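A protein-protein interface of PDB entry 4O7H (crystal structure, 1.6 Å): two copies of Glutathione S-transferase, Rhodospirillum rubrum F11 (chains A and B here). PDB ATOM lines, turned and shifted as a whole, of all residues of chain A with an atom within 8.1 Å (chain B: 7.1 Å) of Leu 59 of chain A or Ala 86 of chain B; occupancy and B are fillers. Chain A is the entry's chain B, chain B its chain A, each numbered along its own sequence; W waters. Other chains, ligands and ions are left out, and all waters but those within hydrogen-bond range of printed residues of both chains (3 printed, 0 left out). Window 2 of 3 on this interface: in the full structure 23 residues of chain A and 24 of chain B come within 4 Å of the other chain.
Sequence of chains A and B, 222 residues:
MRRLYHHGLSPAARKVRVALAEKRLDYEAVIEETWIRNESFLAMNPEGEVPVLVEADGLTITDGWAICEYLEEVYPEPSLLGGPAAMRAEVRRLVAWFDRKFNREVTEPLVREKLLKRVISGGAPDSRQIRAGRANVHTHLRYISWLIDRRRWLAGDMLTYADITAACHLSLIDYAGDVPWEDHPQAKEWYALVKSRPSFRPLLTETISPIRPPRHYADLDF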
ATOM      1  N   ARG A   2      -9.880  18.246  20.960  1.00  0.00           N
ATOM      2  CA  ARG A   2      -8.836  17.340  20.450  1.00  0.00           C
ATOM      3  C   ARG A   2      -8.470  17.771  19.037  1.00  0.00           C
ATOM      4  O   ARG A   2      -9.288  18.357  18.299  1.00  0.00           O
ATOM      5  CB  ARG A   2      -9.287  15.854  20.526  1.00  0.00           C
ATOM      6  CG  ARG A   2     -10.284  15.435  19.486  1.00  0.00           C
ATOM      7  CD  ARG A   2     -10.865  14.011  19.630  1.00  0.00           C
ATOM      8  NE  ARG A   2     -11.299  13.637  20.982  1.00  0.00           N
ATOM      9  CZ  ARG A   2     -12.515  13.872  21.456  1.00  0.00           C
ATOM     10  NH1 ARG A   2     -12.844  13.476  22.672  1.00  0.00           N
ATOM     11  NH2 ARG A   2     -13.409  14.464  20.680  1.00  0.00           N
ATOM     12  N   ARG A   3      -7.232  17.489  18.656  1.00  0.00           N
ATOM     13  CA  ARG A   3      -6.711  17.930  17.380  1.00  0.00           C
ATOM     14  C   ARG A   3      -6.118  16.755  16.678  1.00  0.00           C
ATOM     15  O   ARG A   3      -5.563  15.866  17.321  1.00  0.00           O
ATOM     16  CB  ARG A   3      -5.587  18.955  17.573  1.00  0.00           C
ATOM     17  CG  ARG A   3      -5.856  20.057  18.567  1.00  0.00           C
ATOM     18  CD  ARG A   3      -4.586  20.854  18.819  1.00  0.00           C
ATOM     19  NE  ARG A   3      -4.234  21.700  17.685  1.00  0.00           N
ATOM     20  CZ  ARG A   3      -4.463  23.004  17.639  1.00  0.00           C
ATOM     21  NH1 ARG A   3      -5.050  23.605  18.659  1.00  0.00           N
ATOM     22  NH2 ARG A   3      -4.106  23.712  16.573  1.00  0.00           N
ATOM     23  N   VAL A  52      -1.241  12.254  13.885  1.00  0.00           N
ATOM     24  CA  VAL A  52      -1.015  12.355  15.326  1.00  0.00           C
ATOM     25  C   VAL A  52      -2.278  12.946  15.952  1.00  0.00           C
ATOM     26  O   VAL A  52      -2.742  14.014  15.499  1.00  0.00           O
ATOM     27  CB  VAL A  52       0.182  13.279  15.609  1.00  0.00           C
ATOM     28  CG1 VAL A  52       0.411  13.385  17.115  1.00  0.00           C
ATOM     29  CG2 VAL A  52       1.426  12.718  14.938  1.00  0.00           C
ATOM     30  N   LEU A  53      -2.814  12.307  16.970  1.00  0.00           N
ATOM     31  CA  LEU A  53      -3.979  12.785  17.704  1.00  0.00           C
ATOM     32  C   LEU A  53      -3.536  13.386  19.027  1.00  0.00           C
ATOM     33  O   LEU A  53      -2.773  12.748  19.751  1.00  0.00           O
ATOM     34  CB  LEU A  53      -4.959  11.659  17.945  1.00  0.00           C
ATOM     35  CG  LEU A  53      -6.211  11.985  18.763  1.00  0.00           C
ATOM     36  CD1 LEU A  53      -7.173  12.833  18.002  1.00  0.00           C
ATOM     37  CD2 LEU A  53      -6.857  10.672  19.203  1.00  0.00           C
ATOM     38  N   VAL A  54      -4.000  14.616  19.328  1.00  0.00           N
ATOM     39  CA  VAL A  54      -3.717  15.208  20.623  1.00  0.00           C
ATOM     40  C   VAL A  54      -5.064  15.502  21.316  1.00  0.00           C
ATOM     41  O   VAL A  54      -5.890  16.325  20.844  1.00  0.00           O
ATOM     42  CB  VAL A  54      -2.840  16.484  20.499  1.00  0.00           C
ATOM     43  CG1 VAL A  54      -2.434  16.964  21.882  1.00  0.00           C
ATOM     44  CG2 VAL A  54      -1.628  16.250  19.612  1.00  0.00           C
ATOM     45  N   GLU A  55      -5.302  14.816  22.416  1.00  0.00           N
ATOM     46  CA  GLU A  55      -6.514  15.025  23.168  1.00  0.00           C
ATOM     47  C   GLU A  55      -6.429  16.415  23.839  1.00  0.00           C
ATOM     48  O   GLU A  55      -5.337  16.985  24.016  1.00  0.00           O
ATOM     49  CB  GLU A  55      -6.745  13.925  24.202  1.00  0.00           C
ATOM     50  CG  GLU A  55      -6.979  12.511  23.624  1.00  0.00           C
ATOM     51  CD  GLU A  55      -8.401  12.261  23.193  1.00  0.00           C
ATOM     52  OE1 GLU A  55      -9.099  13.209  22.779  1.00  0.00           O
ATOM     53  OE2 GLU A  55      -8.846  11.099  23.302  1.00  0.00           O
ATOM     54  N   ALA A  56      -7.581  16.929  24.216  1.00  0.00           N
ATOM     55  CA  ALA A  56      -7.660  18.228  24.924  1.00  0.00           C
ATOM     56  C   ALA A  56      -6.731  18.321  26.134  1.00  0.00           C
ATOM     57  O   ALA A  56      -6.203  19.397  26.421  1.00  0.00           O
ATOM     58  CB  ALA A  56      -9.103  18.497  25.333  1.00  0.00           C
ATOM     59  N   ASP A  57      -6.515  17.227  26.850  1.00  0.00           N
ATOM     60  CA  ASP A  57      -5.617  17.251  28.019  1.00  0.00           C
ATOM     61  C   ASP A  57      -4.142  17.047  27.647  1.00  0.00           C
ATOM     62  O   ASP A  57      -3.296  16.858  28.530  1.00  0.00           O
ATOM     63  CB  ASP A  57      -6.044  16.226  29.084  1.00  0.00           C
ATOM     64  CG  ASP A  57      -5.732  14.773  28.690  1.00  0.00           C
ATOM     65  OD1 ASP A  57      -5.335  14.518  27.532  1.00  0.00           O
ATOM     66  OD2 ASP A  57      -5.874  13.863  29.544  1.00  0.00           O
ATOM     67  N   GLY A  58      -3.839  17.031  26.349  1.00  0.00           N
ATOM     68  CA  GLY A  58      -2.473  16.895  25.869  1.00  0.00           C
ATOM     69  C   GLY A  58      -1.980  15.489  25.546  1.00  0.00           C
ATOM     70  O   GLY A  58      -0.884  15.330  25.010  1.00  0.00           O
ATOM     71  N   LEU A  59      -2.765  14.468  25.873  1.00  0.00           N
ATOM     72  CA  LEU A  59      -2.362  13.089  25.567  1.00  0.00           C
ATOM     73  C   LEU A  59      -2.202  12.957  24.055  1.00  0.00           C
ATOM     74  O   LEU A  59      -3.104  13.286  23.332  1.00  0.00           O
ATOM     75  CB  LEU A  59      -3.389  12.079  26.075  1.00  0.00           C
ATOM     76  CG  LEU A  59      -3.009  10.636  25.770  1.00  0.00           C
ATOM     77  CD1 LEU A  59      -1.755  10.215  26.521  1.00  0.00           C
ATOM     78  CD2 LEU A  59      -4.194   9.728  26.098  1.00  0.00           C
ATOM     79  N   THR A  60      -1.056  12.460  23.618  1.00  0.00           N
ATOM     80  CA  THR A  60      -0.643  12.466  22.207  1.00  0.00           C
ATOM     81  C   THR A  60      -0.515  11.031  21.748  1.00  0.00           C
ATOM     82  O   THR A  60       0.287  10.253  22.301  1.00  0.00           O
ATOM     83  CB  THR A  60       0.707  13.184  22.054  1.00  0.00           C
ATOM     84  OG1 THR A  60       0.559  14.547  22.472  1.00  0.00           O
ATOM     85  CG2 THR A  60       1.175  13.205  20.641  1.00  0.00           C
ATOM     86  N   ILE A  61      -1.334  10.655  20.757  1.00  0.00           N
ATOM     87  CA  ILE A  61      -1.349   9.296  20.228  1.00  0.00           C
ATOM     88  C   ILE A  61      -0.874   9.337  18.774  1.00  0.00           C
ATOM     89  O   ILE A  61      -1.402  10.095  17.943  1.00  0.00           O
ATOM     90  CB  ILE A  61      -2.765   8.699  20.279  1.00  0.00           C
ATOM     91  CG1 ILE A  61      -3.445   8.940  21.656  1.00  0.00           C
ATOM     92  CG2 ILE A  61      -2.741   7.211  19.859  1.00  0.00           C
ATOM     93  CD1 ILE A  61      -2.780   8.302  22.852  1.00  0.00           C
ATOM     94  N   THR A  62       0.167   8.554  18.486  1.00  0.00           N
ATOM     95  CA  THR A  62       0.870   8.620  17.246  1.00  0.00           C
ATOM     96  C   THR A  62       0.741   7.279  16.500  1.00  0.00           C
ATOM     97  O   THR A  62       0.772   6.214  17.142  1.00  0.00           O
ATOM     98  CB  THR A  62       2.342   8.892  17.569  1.00  0.00           C
ATOM     99  OG1 THR A  62       2.463  10.184  18.168  1.00  0.00           O
ATOM    100  CG2 THR A  62       3.177   8.776  16.367  1.00  0.00           C
ATOM    101  N   TYR A  70      -6.679   2.911  20.002  1.00  0.00           N
ATOM    102  CA  TYR A  70      -6.934   3.799  21.137  1.00  0.00           C
ATOM    103  C   TYR A  70      -8.357   4.266  21.115  1.00  0.00           C
ATOM    104  O   TYR A  70      -9.043   4.206  22.152  1.00  0.00           O
ATOM    105  CB  TYR A  70      -6.000   4.994  21.064  1.00  0.00           C
ATOM    106  CG  TYR A  70      -6.342   6.151  21.985  1.00  0.00           C
ATOM    107  CD1 TYR A  70      -5.951   6.157  23.310  1.00  0.00           C
ATOM    108  CD2 TYR A  70      -7.100   7.211  21.507  1.00  0.00           C
ATOM    109  CE1 TYR A  70      -6.295   7.249  24.144  1.00  0.00           C
ATOM    110  CE2 TYR A  70      -7.430   8.295  22.348  1.00  0.00           C
ATOM    111  CZ  TYR A  70      -7.004   8.275  23.635  1.00  0.00           C
ATOM    112  OH  TYR A  70      -7.377   9.311  24.514  1.00  0.00           O
ATOM    113  N   GLU A  73     -10.743   1.663  22.334  1.00  0.00           N
ATOM    114  CA  GLU A  73     -10.569   1.381  23.764  1.00  0.00           C
ATOM    115  C   GLU A  73     -11.239   2.466  24.596  1.00  0.00           C
ATOM    116  O   GLU A  73     -11.897   2.160  25.579  1.00  0.00           O
ATOM    117  CB  GLU A  73      -9.098   1.352  24.126  1.00  0.00           C
ATOM    118  CG  GLU A  73      -8.391   0.090  23.675  1.00  0.00           C
ATOM    119  CD  GLU A  73      -6.883   0.109  23.880  1.00  0.00           C
ATOM    120  OE1 GLU A  73      -6.343   0.964  24.591  1.00  0.00           O
ATOM    121  OE2 GLU A  73      -6.223  -0.764  23.305  1.00  0.00           O
ATOM    122  N   VAL A  74     -11.054   3.727  24.207  1.00  0.00           N
ATOM    123  CA  VAL A  74     -11.545   4.882  25.001  1.00  0.00           C
ATOM    124  C   VAL A  74     -12.958   5.353  24.652  1.00  0.00           C
ATOM    125  O   VAL A  74     -13.708   5.817  25.541  1.00  0.00           O
ATOM    126  CB  VAL A  74     -10.513   6.020  24.890  1.00  0.00           C
ATOM    127  CG1 VAL A  74     -10.946   7.256  25.658  1.00  0.00           C
ATOM    128  CG2 VAL A  74      -9.162   5.533  25.391  1.00  0.00           C
ATOM    129  N   TYR A  75     -13.374   5.146  23.410  1.00  0.00           N
ATOM    130  CA  TYR A  75     -14.665   5.554  22.883  1.00  0.00           C
ATOM    131  C   TYR A  75     -15.315   4.331  22.187  1.00  0.00           C
ATOM    132  O   TYR A  75     -15.369   4.253  20.972  1.00  0.00           O
ATOM    133  CB  TYR A  75     -14.480   6.684  21.906  1.00  0.00           C
ATOM    134  CG  TYR A  75     -13.690   7.857  22.432  1.00  0.00           C
ATOM    135  CD1 TYR A  75     -14.250   8.783  23.300  1.00  0.00           C
ATOM    136  CD2 TYR A  75     -12.385   8.061  22.044  1.00  0.00           C
ATOM    137  CE1 TYR A  75     -13.518   9.866  23.762  1.00  0.00           C
ATOM    138  CE2 TYR A  75     -11.638   9.107  22.517  1.00  0.00           C
ATOM    139  CZ  TYR A  75     -12.204  10.020  23.390  1.00  0.00           C
ATOM    140  OH  TYR A  75     -11.428  11.088  23.820  1.00  0.00           O
ATOM    141  N   GLY B  83      -1.505  -1.750  30.447  1.00  0.00           N
ATOM    142  CA  GLY B  83      -2.830  -1.561  31.030  1.00  0.00           C
ATOM    143  C   GLY B  83      -3.455  -0.247  30.620  1.00  0.00           C
ATOM    144  O   GLY B  83      -4.472  -0.233  29.938  1.00  0.00           O
ATOM    145  N   PRO B  84      -2.846   0.875  31.028  1.00  0.00           N
ATOM    146  CA  PRO B  84      -3.512   2.122  30.680  1.00  0.00           C
ATOM    147  C   PRO B  84      -3.500   2.397  29.167  1.00  0.00           C
ATOM    148  O   PRO B  84      -2.543   2.036  28.486  1.00  0.00           O
ATOM    149  CB  PRO B  84      -2.704   3.200  31.440  1.00  0.00           C
ATOM    150  CG  PRO B  84      -1.636   2.490  32.190  1.00  0.00           C
ATOM    151  CD  PRO B  84      -1.548   1.061  31.692  1.00  0.00           C
ATOM    152  N   ALA B  85      -4.548   3.013  28.649  1.00  0.00           N
ATOM    153  CA  ALA B  85      -4.624   3.335  27.213  1.00  0.00           C
ATOM    154  C   ALA B  85      -3.387   4.037  26.686  1.00  0.00           C
ATOM    155  O   ALA B  85      -2.943   3.800  25.558  1.00  0.00           O
ATOM    156  CB  ALA B  85      -5.859   4.162  26.913  1.00  0.00           C
ATOM    157  N   ALA B  86      -2.846   4.966  27.461  1.00  0.00           N
ATOM    158  CA  ALA B  86      -1.659   5.710  27.061  1.00  0.00           C
ATOM    159  C   ALA B  86      -0.435   4.835  26.883  1.00  0.00           C
ATOM    160  O   ALA B  86       0.360   5.063  25.976  1.00  0.00           O
ATOM    161  CB  ALA B  86      -1.344   6.823  28.073  1.00  0.00           C
ATOM    162  N   MET B  87      -0.275   3.841  27.748  1.00  0.00           N
ATOM    163  CA  MET B  87       0.857   2.950  27.652  1.00  0.00           C
ATOM    164  C   MET B  87       0.676   2.081  26.425  1.00  0.00           C
ATOM    165  O   MET B  87       1.604   1.918  25.635  1.00  0.00           O
ATOM    166  CB  MET B  87       0.977   2.057  28.862  1.00  0.00           C
ATOM    167  CG  MET B  87       2.004   0.962  28.638  1.00  0.00           C
ATOM    168  SD  MET B  87       2.456   0.179  30.174  1.00  0.00           S
ATOM    169  CE  MET B  87       3.745  -0.863  29.509  1.00  0.00           C
ATOM    170  N   ARG B  88      -0.527   1.538  26.272  1.00  0.00           N
ATOM    171  CA  ARG B  88      -0.819   0.673  25.083  1.00  0.00           C
ATOM    172  C   ARG B  88      -0.567   1.435  23.787  1.00  0.00           C
ATOM    173  O   ARG B  88      -0.030   0.881  22.815  1.00  0.00           O
ATOM    174  CB  ARG B  88      -2.246   0.150  25.140  1.00  0.00           C
ATOM    175  CG  ARG B  88      -2.442  -0.791  26.293  1.00  0.00           C
ATOM    176  CD  ARG B  88      -3.864  -0.880  26.702  1.00  0.00           C
ATOM    177  NE  ARG B  88      -4.654  -1.592  25.744  1.00  0.00           N
ATOM    178  CZ  ARG B  88      -4.859  -2.901  25.751  1.00  0.00           C
ATOM    179  NH1 ARG B  88      -4.278  -3.661  26.664  1.00  0.00           N
ATOM    180  NH2 ARG B  88      -5.652  -3.440  24.834  1.00  0.00           N
ATOM    181  N   ALA B  89      -0.932   2.719  23.751  1.00  0.00           N
ATOM    182  CA  ALA B  89      -0.666   3.535  22.578  1.00  0.00           C
ATOM    183  C   ALA B  89       0.840   3.685  22.292  1.00  0.00           C
ATOM    184  O   ALA B  89       1.228   3.761  21.132  1.00  0.00           O
ATOM    185  CB  ALA B  89      -1.309   4.905  22.746  1.00  0.00           C
ATOM    186  N   GLU B  90       1.666   3.801  23.337  1.00  0.00           N
ATOM    187  CA  GLU B  90       3.115   3.919  23.181  1.00  0.00           C
ATOM    188  C   GLU B  90       3.688   2.596  22.654  1.00  0.00           C
ATOM    189  O   GLU B  90       4.547   2.571  21.740  1.00  0.00           O
ATOM    190  CB  GLU B  90       3.751   4.329  24.522  1.00  0.00           C
ATOM    191  CG  GLU B  90       5.257   4.401  24.539  1.00  0.00           C
ATOM    192  CD  GLU B  90       5.874   5.454  23.633  1.00  0.00           C
ATOM    193  OE1 GLU B  90       5.145   6.301  23.066  1.00  0.00           O
ATOM    194  OE2 GLU B  90       7.127   5.433  23.462  1.00  0.00           O
ATOM    195  N   VAL B  91       3.192   1.496  23.202  1.00  0.00           N
ATOM    196  CA  VAL B  91       3.593   0.175  22.669  1.00  0.00           C
ATOM    197  C   VAL B  91       3.279   0.099  21.171  1.00  0.00           C
ATOM    198  O   VAL B  91       4.135  -0.323  20.341  1.00  0.00           O
ATOM    199  CB  VAL B  91       2.899  -0.977  23.403  1.00  0.00           C
ATOM    200  CG1 VAL B  91       3.222  -2.303  22.712  1.00  0.00           C
ATOM    201  CG2 VAL B  91       3.340  -1.023  24.853  1.00  0.00           C
ATOM    202  N   ALA B 155       9.092   0.437  25.756  1.00  0.00           N
ATOM    203  CA  ALA B 155       7.828   1.164  25.873  1.00  0.00           C
ATOM    204  C   ALA B 155       7.486   1.551  27.279  1.00  0.00           C
ATOM    205  O   ALA B 155       6.414   2.149  27.503  1.00  0.00           O
ATOM    206  CB  ALA B 155       6.677   0.356  25.279  1.00  0.00           C
HETATM  207  O   HOH W   1       1.022   6.716  20.522  1.00  0.00           O
HETATM  208  O   HOH W   2      -4.485   2.739  23.471  1.00  0.00           O
HETATM  209  O   HOH W   3      -7.490  -3.227  22.566  1.00  0.00           O
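The side-chain carboxylate (OE2) of Glu 73 of chain A is in salt-bridge range of the guanidinium group (NE) of Arg 88 of chain B.
Among the printed residues, merely in contact across the chains: Ile 61 of chain A with Ala 89 of chain B (3.7 Å), Leu 59 of chain A with Ala 86 of chain B (3.8 Å), Val 74 of chain A with Ala 85 of chain B (3.9 Å) and Glu 73 of chain A with Ala 85 of chain B (3.9 Å).
Printed residues of chain A that touch a printed residue of chain B: Leu 59, Ile 61, Glu 73 and Val 74. Hydrophobic or aromatic side chains of chain A that line the printed part of chain B: Leu 59, Ile 61 and Val 74. Hydrophobic or aromatic side chains of chain B that line the printed part of chain A: Ala 85, Ala 86 and Ala 89. Among the printed residues, 5 pairs touch across the chains.
Water W2 bridges O of Ala 85 of chain B (2.8 Å) and OE1 of Glu 73 of chain A (2.8 Å). Water W3 lies within hydrogen-bond range of the side-chain carboxylate of Glu 73 of chain A and the guanidinium group of Arg 88 of chain B. Water W1 bridges the backbone NH (N) of Thr 62 of chain A and the backbone carbonyl oxygen (O) of Ala 89 of chain B.
No position is printed for both chains.
Of chain B, only Ala 86 comes within 4 Å of Leu 59 of chain A. Ala 86 of chain B touches just one residue of chain A: Leu 59 (3.8 Å). No residue of chain B comes within 4 Å of Gly 58 of chain A. Of chain A, only Glu 73 and Val 74 come within 4 Å of Ala 85 of chain B. Of the printed residues of chain A, Ala 89 of chain B touches Ile 61. Printed residues of chain B within 4 Å of Ile 61 of chain A: Ala 89 (3.7 Å). Glu 55 of chain A touches none of the printed residues of chain B. The nearest residue of chain A that does not touch Ala 86 of chain B is Ile 61 of chain A (5.1 Å).
The side-chain carboxylate (OD1) of Asp 57 of chain A lies within hydrogen-bond range of the backbone NH (N) of Leu 59 of chain A (3.1 Å). The backbone NH of Ile 61 of chain A sits at hydrogen-bond distance from the backbone carbonyl oxygen of Leu 53 of chain A, 2.7 Å away.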
